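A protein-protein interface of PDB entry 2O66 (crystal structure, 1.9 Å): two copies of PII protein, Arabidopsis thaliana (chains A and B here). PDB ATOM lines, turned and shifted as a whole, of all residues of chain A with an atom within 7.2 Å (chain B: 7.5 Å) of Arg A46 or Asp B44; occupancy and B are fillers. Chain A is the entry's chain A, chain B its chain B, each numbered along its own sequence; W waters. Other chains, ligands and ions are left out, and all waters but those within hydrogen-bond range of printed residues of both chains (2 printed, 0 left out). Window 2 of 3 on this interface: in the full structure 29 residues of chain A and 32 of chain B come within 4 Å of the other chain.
Water W2 lies within hydrogen-bond range of the side-chain carboxylate (OD2) of Asp B44 (2.7 Å) and the guanidinium group (NH1) of Arg A46 (3.4 Å). Water W1 lies within hydrogen-bond range of the backbone NH of Asp B44 (2.7 Å), the backbone carbonyl oxygen of Asp A44 (3.1 Å) and the guanidinium group of Arg A46 (3.5 Å).
N of Val A45 is in hydrogen-bond range of O of Lys A71 (3.0 Å). The backbone carbonyl oxygen (O) of Val A69 lies within hydrogen-bond range of the backbone NH (N) of Gly A47 (2.8 Å). The backbone carbonyl oxygen of Thr B41 lies within hydrogen-bond range of the backbone NH of Glu B75 (2.7 Å). O of Ser B43 lies within hydrogen-bond range of N of Lys B73 (2.8 Å).
Arg A46 touches just these residues of chain B: Val B40, Thr B41, Val B42 and Asp B44. Of the printed residues of chain B, Gly A49 touches Val B40 (3.2 Å). Of the printed residues of chain A, Val B42 touches Val A45 (3.4 Å), Arg A46 (2.7 Å) and Phe A48 (3.8 Å). Of the printed residues of chain A, Ser B43 touches Asp A44 and Val A45. Asp B44 touches just one residue of chain A: Arg A46 (2.9 Å). The nearest residue of chain B that does not touch Arg A46 is Val B72 (4.2 Å). The nearest residue of chain A that does not touch Asp B44 is Asp A44 (5.2 Å). The nearest printed residue of chain B that does not touch Asp A44 is Val B42 (4.8 Å).
Arg A46 touches Asp B44, but with the chains exchanged Asp A44 does not touch Arg B46 (10.5 Å). Positions printed for both chains: 44, 45, 46, 70, 71 and 72.
N of Arg A46 sits at hydrogen-bond distance from O of Val B42. The guanidinium group of Arg A46 is in salt-bridge range of the side-chain carboxylate of Asp B44 (2.9 Å). The backbone NH (N) of Phe A48 is in hydrogen-bond range of the backbone carbonyl oxygen (O) of Val B40 (3.4 Å). The backbone carbonyl oxygen (O) of Val B40 sits at hydrogen-bond distance from the backbone NH (N) of Gly A49, 3.3 Å away.
Among the printed residues, pairs that only touch across the chains: Val A45 with Val B42 (3.4 Å), Gly A47 with Val B40 (3.6 Å), Val A45 with Thr B41 (3.7 Å), Arg A46 with Thr B41 (3.7 Å), Arg A46 with Val B40 (3.7 Å), Phe A48 with Val B42 (3.8 Å), Asp A44 with Ser B43 (3.9 Å) and Val A45 with Ser B43 (3.9 Å).
Printed residues of chain A that touch a printed residue of chain B: Asp A44, Val A45, Arg A46, Gly A47, Phe A48 and Gly A49. Hydrophobic or aromatic side chains of chain B within 4 Å of the printed part of chain A: Val B42.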
ATOM      1  N   ILE A  19       2.942 -11.482   0.668  1.00  0.00           N
ATOM      2  CA  ILE A  19       1.974 -11.555   1.760  1.00  0.00           C
ATOM      3  C   ILE A  19       0.604 -11.543   1.114  1.00  0.00           C
ATOM      4  O   ILE A  19       0.177 -10.508   0.614  1.00  0.00           O
ATOM      5  CB  ILE A  19       2.086 -10.344   2.726  1.00  0.00           C
ATOM      6  CG1 ILE A  19       3.546 -10.030   3.073  1.00  0.00           C
ATOM      7  CG2 ILE A  19       1.235 -10.566   3.985  1.00  0.00           C
ATOM      8  CD1 ILE A  19       4.252 -11.093   3.859  1.00  0.00           C
ATOM      9  N   ASP A  44       2.309 -18.292   8.556  1.00  0.00           N
ATOM     10  CA  ASP A  44       1.139 -17.493   8.869  1.00  0.00           C
ATOM     11  C   ASP A  44       1.559 -16.171   9.474  1.00  0.00           C
ATOM     12  O   ASP A  44       2.463 -16.113  10.316  1.00  0.00           O
ATOM     13  CB  ASP A  44       0.207 -18.259   9.806  1.00  0.00           C
ATOM     14  CG  ASP A  44      -0.261 -19.569   9.205  1.00  0.00           C
ATOM     15  OD1 ASP A  44      -0.722 -19.562   8.042  1.00  0.00           O
ATOM     16  OD2 ASP A  44      -0.151 -20.607   9.887  1.00  0.00           O
ATOM     17  N   VAL A  45       0.922 -15.104   9.007  1.00  0.00           N
ATOM     18  CA  VAL A  45       1.166 -13.777   9.536  1.00  0.00           C
ATOM     19  C   VAL A  45      -0.170 -13.093   9.821  1.00  0.00           C
ATOM     20  O   VAL A  45      -1.225 -13.541   9.355  1.00  0.00           O
ATOM     21  CB  VAL A  45       2.067 -12.914   8.600  1.00  0.00           C
ATOM     22  CG1 VAL A  45       3.458 -13.540   8.452  1.00  0.00           C
ATOM     23  CG2 VAL A  45       1.431 -12.708   7.236  1.00  0.00           C
ATOM     24  N   ARG A  46      -0.115 -12.023  10.602  1.00  0.00           N
ATOM     25  CA  ARG A  46      -1.310 -11.290  10.982  1.00  0.00           C
ATOM     26  C   ARG A  46      -1.153  -9.827  10.610  1.00  0.00           C
ATOM     27  O   ARG A  46      -0.201  -9.166  11.030  1.00  0.00           O
ATOM     28  CB  ARG A  46      -1.585 -11.444  12.481  1.00  0.00           C
ATOM     29  CG  ARG A  46      -1.749 -12.898  12.928  1.00  0.00           C
ATOM     30  CD  ARG A  46      -2.109 -13.016  14.404  1.00  0.00           C
ATOM     31  NE  ARG A  46      -1.045 -12.552  15.300  1.00  0.00           N
ATOM     32  CZ  ARG A  46       0.087 -13.210  15.547  1.00  0.00           C
ATOM     33  NH1 ARG A  46       0.345 -14.372  14.955  1.00  0.00           N
ATOM     34  NH2 ARG A  46       0.974 -12.698  16.387  1.00  0.00           N
ATOM     35  N   GLY A  47      -2.083  -9.336   9.799  1.00  0.00           N
ATOM     36  CA  GLY A  47      -2.140  -7.920   9.485  1.00  0.00           C
ATOM     37  C   GLY A  47      -2.943  -7.221  10.558  1.00  0.00           C
ATOM     38  O   GLY A  47      -4.171  -7.212  10.512  1.00  0.00           O
ATOM     39  N   PHE A  48      -2.247  -6.670  11.551  1.00  0.00           N
ATOM     40  CA  PHE A  48      -2.885  -5.817  12.557  1.00  0.00           C
ATOM     41  C   PHE A  48      -3.071  -4.438  11.952  1.00  0.00           C
ATOM     42  O   PHE A  48      -3.917  -3.652  12.383  1.00  0.00           O
ATOM     43  CB  PHE A  48      -2.056  -5.758  13.838  1.00  0.00           C
ATOM     44  CG  PHE A  48      -2.239  -6.952  14.731  1.00  0.00           C
ATOM     45  CD1 PHE A  48      -3.289  -6.997  15.644  1.00  0.00           C
ATOM     46  CD2 PHE A  48      -1.367  -8.034  14.660  1.00  0.00           C
ATOM     47  CE1 PHE A  48      -3.468  -8.103  16.477  1.00  0.00           C
ATOM     48  CE2 PHE A  48      -1.536  -9.144  15.488  1.00  0.00           C
ATOM     49  CZ  PHE A  48      -2.589  -9.177  16.400  1.00  0.00           C
ATOM     50  N   GLY A  49      -2.251  -4.163  10.943  1.00  0.00           N
ATOM     51  CA  GLY A  49      -2.488  -3.087  10.004  1.00  0.00           C
ATOM     52  C   GLY A  49      -2.548  -3.677   8.605  1.00  0.00           C
ATOM     53  O   GLY A  49      -1.824  -4.627   8.285  1.00  0.00           O
ATOM     54  N   ASP A  66      -8.124  -7.244  19.946  1.00  0.00           N
ATOM     55  CA  ASP A  66      -6.976  -7.480  19.076  1.00  0.00           C
ATOM     56  C   ASP A  66      -7.433  -8.039  17.725  1.00  0.00           C
ATOM     57  O   ASP A  66      -7.324  -9.240  17.468  1.00  0.00           O
ATOM     58  CB  ASP A  66      -5.982  -8.436  19.753  1.00  0.00           C
ATOM     59  CG  ASP A  66      -5.619  -8.001  21.164  1.00  0.00           C
ATOM     60  OD1 ASP A  66      -4.973  -6.942  21.318  1.00  0.00           O
ATOM     61  OD2 ASP A  66      -5.979  -8.721  22.121  1.00  0.00           O
ATOM     62  N   LYS A  67      -7.947  -7.154  16.873  1.00  0.00           N
ATOM     63  CA  LYS A  67      -8.466  -7.548  15.562  1.00  0.00           C
ATOM     64  C   LYS A  67      -7.361  -7.568  14.509  1.00  0.00           C
ATOM     65  O   LYS A  67      -6.494  -6.693  14.499  1.00  0.00           O
ATOM     66  CB  LYS A  67      -9.600  -6.613  15.131  1.00  0.00           C
ATOM     67  CG  LYS A  67     -10.598  -7.248  14.163  1.00  0.00           C
ATOM     68  CD  LYS A  67     -11.784  -6.332  13.841  1.00  0.00           C
ATOM     69  CE  LYS A  67     -12.832  -6.309  14.952  1.00  0.00           C
ATOM     70  NZ  LYS A  67     -12.473  -5.391  16.076  1.00  0.00           N
ATOM     71  N   PHE A  68      -7.392  -8.569  13.631  1.00  0.00           N
ATOM     72  CA  PHE A  68      -6.378  -8.702  12.580  1.00  0.00           C
ATOM     73  C   PHE A  68      -6.910  -9.395  11.333  1.00  0.00           C
ATOM     74  O   PHE A  68      -7.951 -10.059  11.372  1.00  0.00           O
ATOM     75  CB  PHE A  68      -5.139  -9.445  13.109  1.00  0.00           C
ATOM     76  CG  PHE A  68      -5.373 -10.907  13.408  1.00  0.00           C
ATOM     77  CD1 PHE A  68      -5.181 -11.877  12.423  1.00  0.00           C
ATOM     78  CD2 PHE A  68      -5.757 -11.317  14.682  1.00  0.00           C
ATOM     79  CE1 PHE A  68      -5.392 -13.235  12.695  1.00  0.00           C
ATOM     80  CE2 PHE A  68      -5.964 -12.676  14.965  1.00  0.00           C
ATOM     81  CZ  PHE A  68      -5.784 -13.632  13.969  1.00  0.00           C
ATOM     82  N   VAL A  69      -6.193  -9.235  10.226  1.00  0.00           N
ATOM     83  CA  VAL A  69      -6.481 -10.000   9.017  1.00  0.00           C
ATOM     84  C   VAL A  69      -5.463 -11.129   8.869  1.00  0.00           C
ATOM     85  O   VAL A  69      -4.253 -10.904   8.970  1.00  0.00           O
ATOM     86  CB  VAL A  69      -6.540  -9.114   7.732  1.00  0.00           C
ATOM     87  CG1 VAL A  69      -7.723  -8.156   7.795  1.00  0.00           C
ATOM     88  CG2 VAL A  69      -5.246  -8.335   7.526  1.00  0.00           C
ATOM     89  N   ALA A  70      -5.959 -12.346   8.660  1.00  0.00           N
ATOM     90  CA  ALA A  70      -5.094 -13.501   8.448  1.00  0.00           C
ATOM     91  C   ALA A  70      -4.495 -13.436   7.054  1.00  0.00           C
ATOM     92  O   ALA A  70      -5.212 -13.251   6.077  1.00  0.00           O
ATOM     93  CB  ALA A  70      -5.871 -14.801   8.628  1.00  0.00           C
ATOM     94  N   LYS A  71      -3.175 -13.555   6.974  1.00  0.00           N
ATOM     95  CA  LYS A  71      -2.482 -13.630   5.695  1.00  0.00           C
ATOM     96  C   LYS A  71      -1.467 -14.755   5.770  1.00  0.00           C
ATOM     97  O   LYS A  71      -1.176 -15.285   6.854  1.00  0.00           O
ATOM     98  CB  LYS A  71      -1.748 -12.315   5.387  1.00  0.00           C
ATOM     99  CG  LYS A  71      -2.622 -11.093   5.085  1.00  0.00           C
ATOM    100  CD  LYS A  71      -3.189 -11.129   3.668  1.00  0.00           C
ATOM    101  CE  LYS A  71      -3.214  -9.741   3.023  1.00  0.00           C
ATOM    102  NZ  LYS A  71      -4.021  -8.739   3.785  1.00  0.00           N
ATOM    103  N   VAL A  72      -0.924 -15.125   4.616  1.00  0.00           N
ATOM    104  CA  VAL A  72       0.204 -16.039   4.601  1.00  0.00           C
ATOM    105  C   VAL A  72       1.363 -15.383   3.867  1.00  0.00           C
ATOM    106  O   VAL A  72       1.173 -14.757   2.819  1.00  0.00           O
ATOM    107  CB  VAL A  72      -0.136 -17.408   3.965  1.00  0.00           C
ATOM    108  CG1 VAL A  72      -1.109 -18.187   4.853  1.00  0.00           C
ATOM    109  CG2 VAL A  72      -0.705 -17.233   2.557  1.00  0.00           C
ATOM    110  N   PRO B  22       5.445  -9.745  22.877  1.00  0.00           N
ATOM    111  CA  PRO B  22       4.113  -9.933  22.294  1.00  0.00           C
ATOM    112  C   PRO B  22       3.063  -8.954  22.821  1.00  0.00           C
ATOM    113  O   PRO B  22       2.153  -8.581  22.083  1.00  0.00           O
ATOM    114  CB  PRO B  22       3.755 -11.374  22.689  1.00  0.00           C
ATOM    115  CG  PRO B  22       5.064 -12.037  22.919  1.00  0.00           C
ATOM    116  CD  PRO B  22       5.925 -10.973  23.536  1.00  0.00           C
ATOM    117  N   ILE B  25       2.422  -5.262  20.999  1.00  0.00           N
ATOM    118  CA  ILE B  25       1.872  -5.165  19.636  1.00  0.00           C
ATOM    119  C   ILE B  25       1.016  -3.916  19.442  1.00  0.00           C
ATOM    120  O   ILE B  25       1.284  -3.106  18.549  1.00  0.00           O
ATOM    121  CB  ILE B  25       1.040  -6.425  19.225  1.00  0.00           C
ATOM    122  CG1 ILE B  25       1.937  -7.656  19.079  1.00  0.00           C
ATOM    123  CG2 ILE B  25       0.291  -6.177  17.903  1.00  0.00           C
ATOM    124  CD1 ILE B  25       1.185  -8.987  18.974  1.00  0.00           C
ATOM    125  N   VAL B  40       0.958  -2.958   9.594  1.00  0.00           N
ATOM    126  CA  VAL B  40       2.107  -3.731  10.052  1.00  0.00           C
ATOM    127  C   VAL B  40       1.780  -5.223   9.934  1.00  0.00           C
ATOM    128  O   VAL B  40       0.627  -5.634  10.103  1.00  0.00           O
ATOM    129  CB  VAL B  40       2.546  -3.321  11.496  1.00  0.00           C
ATOM    130  CG1 VAL B  40       1.428  -3.547  12.515  1.00  0.00           C
ATOM    131  CG2 VAL B  40       3.827  -4.041  11.920  1.00  0.00           C
ATOM    132  N   THR B  41       2.793  -6.017   9.605  1.00  0.00           N
ATOM    133  CA  THR B  41       2.648  -7.463   9.504  1.00  0.00           C
ATOM    134  C   THR B  41       3.313  -8.095  10.717  1.00  0.00           C
ATOM    135  O   THR B  41       4.468  -7.797  11.017  1.00  0.00           O
ATOM    136  CB  THR B  41       3.274  -7.990   8.194  1.00  0.00           C
ATOM    137  OG1 THR B  41       2.492  -7.534   7.084  1.00  0.00           O
ATOM    138  CG2 THR B  41       3.314  -9.508   8.170  1.00  0.00           C
ATOM    139  N   VAL B  42       2.576  -8.963  11.409  1.00  0.00           N
ATOM    140  CA  VAL B  42       3.033  -9.556  12.669  1.00  0.00           C
ATOM    141  C   VAL B  42       3.049 -11.081  12.597  1.00  0.00           C
ATOM    142  O   VAL B  42       2.125 -11.693  12.058  1.00  0.00           O
ATOM    143  CB  VAL B  42       2.157  -9.070  13.860  1.00  0.00           C
ATOM    144  CG1 VAL B  42       2.513  -9.791  15.157  1.00  0.00           C
ATOM    145  CG2 VAL B  42       2.304  -7.560  14.041  1.00  0.00           C
ATOM    146  N   SER B  43       4.110 -11.685  13.132  1.00  0.00           N
ATOM    147  CA  SER B  43       4.201 -13.145  13.233  1.00  0.00           C
ATOM    148  C   SER B  43       4.845 -13.579  14.544  1.00  0.00           C
ATOM    149  O   SER B  43       5.550 -12.800  15.190  1.00  0.00           O
ATOM    150  CB  SER B  43       4.954 -13.734  12.039  1.00  0.00           C
ATOM    151  OG  SER B  43       6.174 -13.052  11.816  1.00  0.00           O
ATOM    152  N   ASP B  44       4.593 -14.825  14.932  1.00  0.00           N
ATOM    153  CA  ASP B  44       5.139 -15.373  16.167  1.00  0.00           C
ATOM    154  C   ASP B  44       6.520 -15.961  15.946  1.00  0.00           C
ATOM    155  O   ASP B  44       6.741 -16.733  15.008  1.00  0.00           O
ATOM    156  CB  ASP B  44       4.195 -16.431  16.739  1.00  0.00           C
ATOM    157  CG  ASP B  44       2.822 -15.871  17.038  1.00  0.00           C
ATOM    158  OD1 ASP B  44       2.731 -14.946  17.873  1.00  0.00           O
ATOM    159  OD2 ASP B  44       1.839 -16.338  16.426  1.00  0.00           O
ATOM    160  N   VAL B  45       7.455 -15.568  16.803  1.00  0.00           N
ATOM    161  CA  VAL B  45       8.798 -16.144  16.799  1.00  0.00           C
ATOM    162  C   VAL B  45       9.185 -16.542  18.226  1.00  0.00           C
ATOM    163  O   VAL B  45       8.520 -16.152  19.188  1.00  0.00           O
ATOM    164  CB  VAL B  45       9.875 -15.197  16.168  1.00  0.00           C
ATOM    165  CG1 VAL B  45       9.567 -14.913  14.696  1.00  0.00           C
ATOM    166  CG2 VAL B  45      10.012 -13.900  16.956  1.00  0.00           C
ATOM    167  N   ARG B  46      10.245 -17.334  18.348  1.00  0.00           N
ATOM    168  CA  ARG B  46      10.722 -17.801  19.648  1.00  0.00           C
ATOM    169  C   ARG B  46      12.217 -17.523  19.785  1.00  0.00           C
ATOM    170  O   ARG B  46      12.982 -17.759  18.854  1.00  0.00           O
ATOM    171  CB  ARG B  46      10.456 -19.306  19.819  1.00  0.00           C
ATOM    172  CG  ARG B  46       9.021 -19.744  19.528  1.00  0.00           C
ATOM    173  CD  ARG B  46       8.780 -21.233  19.806  1.00  0.00           C
ATOM    174  NE  ARG B  46       9.494 -22.153  18.911  1.00  0.00           N
ATOM    175  CZ  ARG B  46       9.137 -22.441  17.658  1.00  0.00           C
ATOM    176  NH1 ARG B  46       8.082 -21.865  17.100  1.00  0.00           N
ATOM    177  NH2 ARG B  46       9.850 -23.305  16.948  1.00  0.00           N
ATOM    178  N   ALA B  70       8.859 -16.168  24.177  1.00  0.00           N
ATOM    179  CA  ALA B  70       7.910 -15.736  23.155  1.00  0.00           C
ATOM    180  C   ALA B  70       8.199 -14.306  22.707  1.00  0.00           C
ATOM    181  O   ALA B  70       8.402 -13.409  23.526  1.00  0.00           O
ATOM    182  CB  ALA B  70       6.481 -15.869  23.656  1.00  0.00           C
ATOM    183  N   LYS B  71       8.251 -14.116  21.394  1.00  0.00           N
ATOM    184  CA  LYS B  71       8.424 -12.796  20.805  1.00  0.00           C
ATOM    185  C   LYS B  71       7.476 -12.666  19.621  1.00  0.00           C
ATOM    186  O   LYS B  71       6.897 -13.650  19.162  1.00  0.00           O
ATOM    187  CB  LYS B  71       9.874 -12.590  20.335  1.00  0.00           C
ATOM    188  CG  LYS B  71      10.923 -12.415  21.435  1.00  0.00           C
ATOM    189  CD  LYS B  71      10.866 -11.016  22.062  1.00  0.00           C
ATOM    190  CE  LYS B  71      12.233 -10.544  22.558  1.00  0.00           C
ATOM    191  NZ  LYS B  71      12.865 -11.490  23.525  1.00  0.00           N
ATOM    192  N   VAL B  72       7.306 -11.449  19.131  1.00  0.00           N
ATOM    193  CA  VAL B  72       6.610 -11.248  17.871  1.00  0.00           C
ATOM    194  C   VAL B  72       7.514 -10.458  16.931  1.00  0.00           C
ATOM    195  O   VAL B  72       8.239  -9.556  17.364  1.00  0.00           O
ATOM    196  CB  VAL B  72       5.229 -10.559  18.041  1.00  0.00           C
ATOM    197  CG1 VAL B  72       4.236 -11.495  18.752  1.00  0.00           C
ATOM    198  CG2 VAL B  72       5.357  -9.237  18.778  1.00  0.00           C
ATOM    199  N   LYS B  73       7.492 -10.839  15.658  1.00  0.00           N
ATOM    200  CA  LYS B  73       8.187 -10.108  14.616  1.00  0.00           C
ATOM    201  C   LYS B  73       7.192  -9.165  13.966  1.00  0.00           C
ATOM    202  O   LYS B  73       6.141  -9.597  13.499  1.00  0.00           O
ATOM    203  CB  LYS B  73       8.748 -11.066  13.563  1.00  0.00           C
ATOM    204  CG  LYS B  73       9.552 -10.381  12.464  1.00  0.00           C
ATOM    205  CD  LYS B  73       9.858 -11.319  11.304  1.00  0.00           C
ATOM    206  CE  LYS B  73      10.979 -12.300  11.631  1.00  0.00           C
ATOM    207  NZ  LYS B  73      11.176 -13.253  10.500  1.00  0.00           N
ATOM    208  N   GLU B  75       6.838  -6.472  10.907  1.00  0.00           N
ATOM    209  CA  GLU B  75       7.487  -6.133   9.647  1.00  0.00           C
ATOM    210  C   GLU B  75       6.776  -4.974   8.978  1.00  0.00           C
ATOM    211  O   GLU B  75       5.551  -4.985   8.825  1.00  0.00           O
ATOM    212  CB  GLU B  75       7.488  -7.333   8.701  1.00  0.00           C
ATOM    213  CG  GLU B  75       8.325  -8.508   9.161  1.00  0.00           C
ATOM    214  CD  GLU B  75       8.166  -9.697   8.241  1.00  0.00           C
ATOM    215  OE1 GLU B  75       8.832  -9.733   7.188  1.00  0.00           O
ATOM    216  OE2 GLU B  75       7.371 -10.597   8.569  1.00  0.00           O
HETATM  217  O   HOH W   1       2.820 -16.226  13.367  1.00  0.00           O
HETATM  218  O   HOH W   2      -0.610 -16.359  17.570  1.00  0.00           O
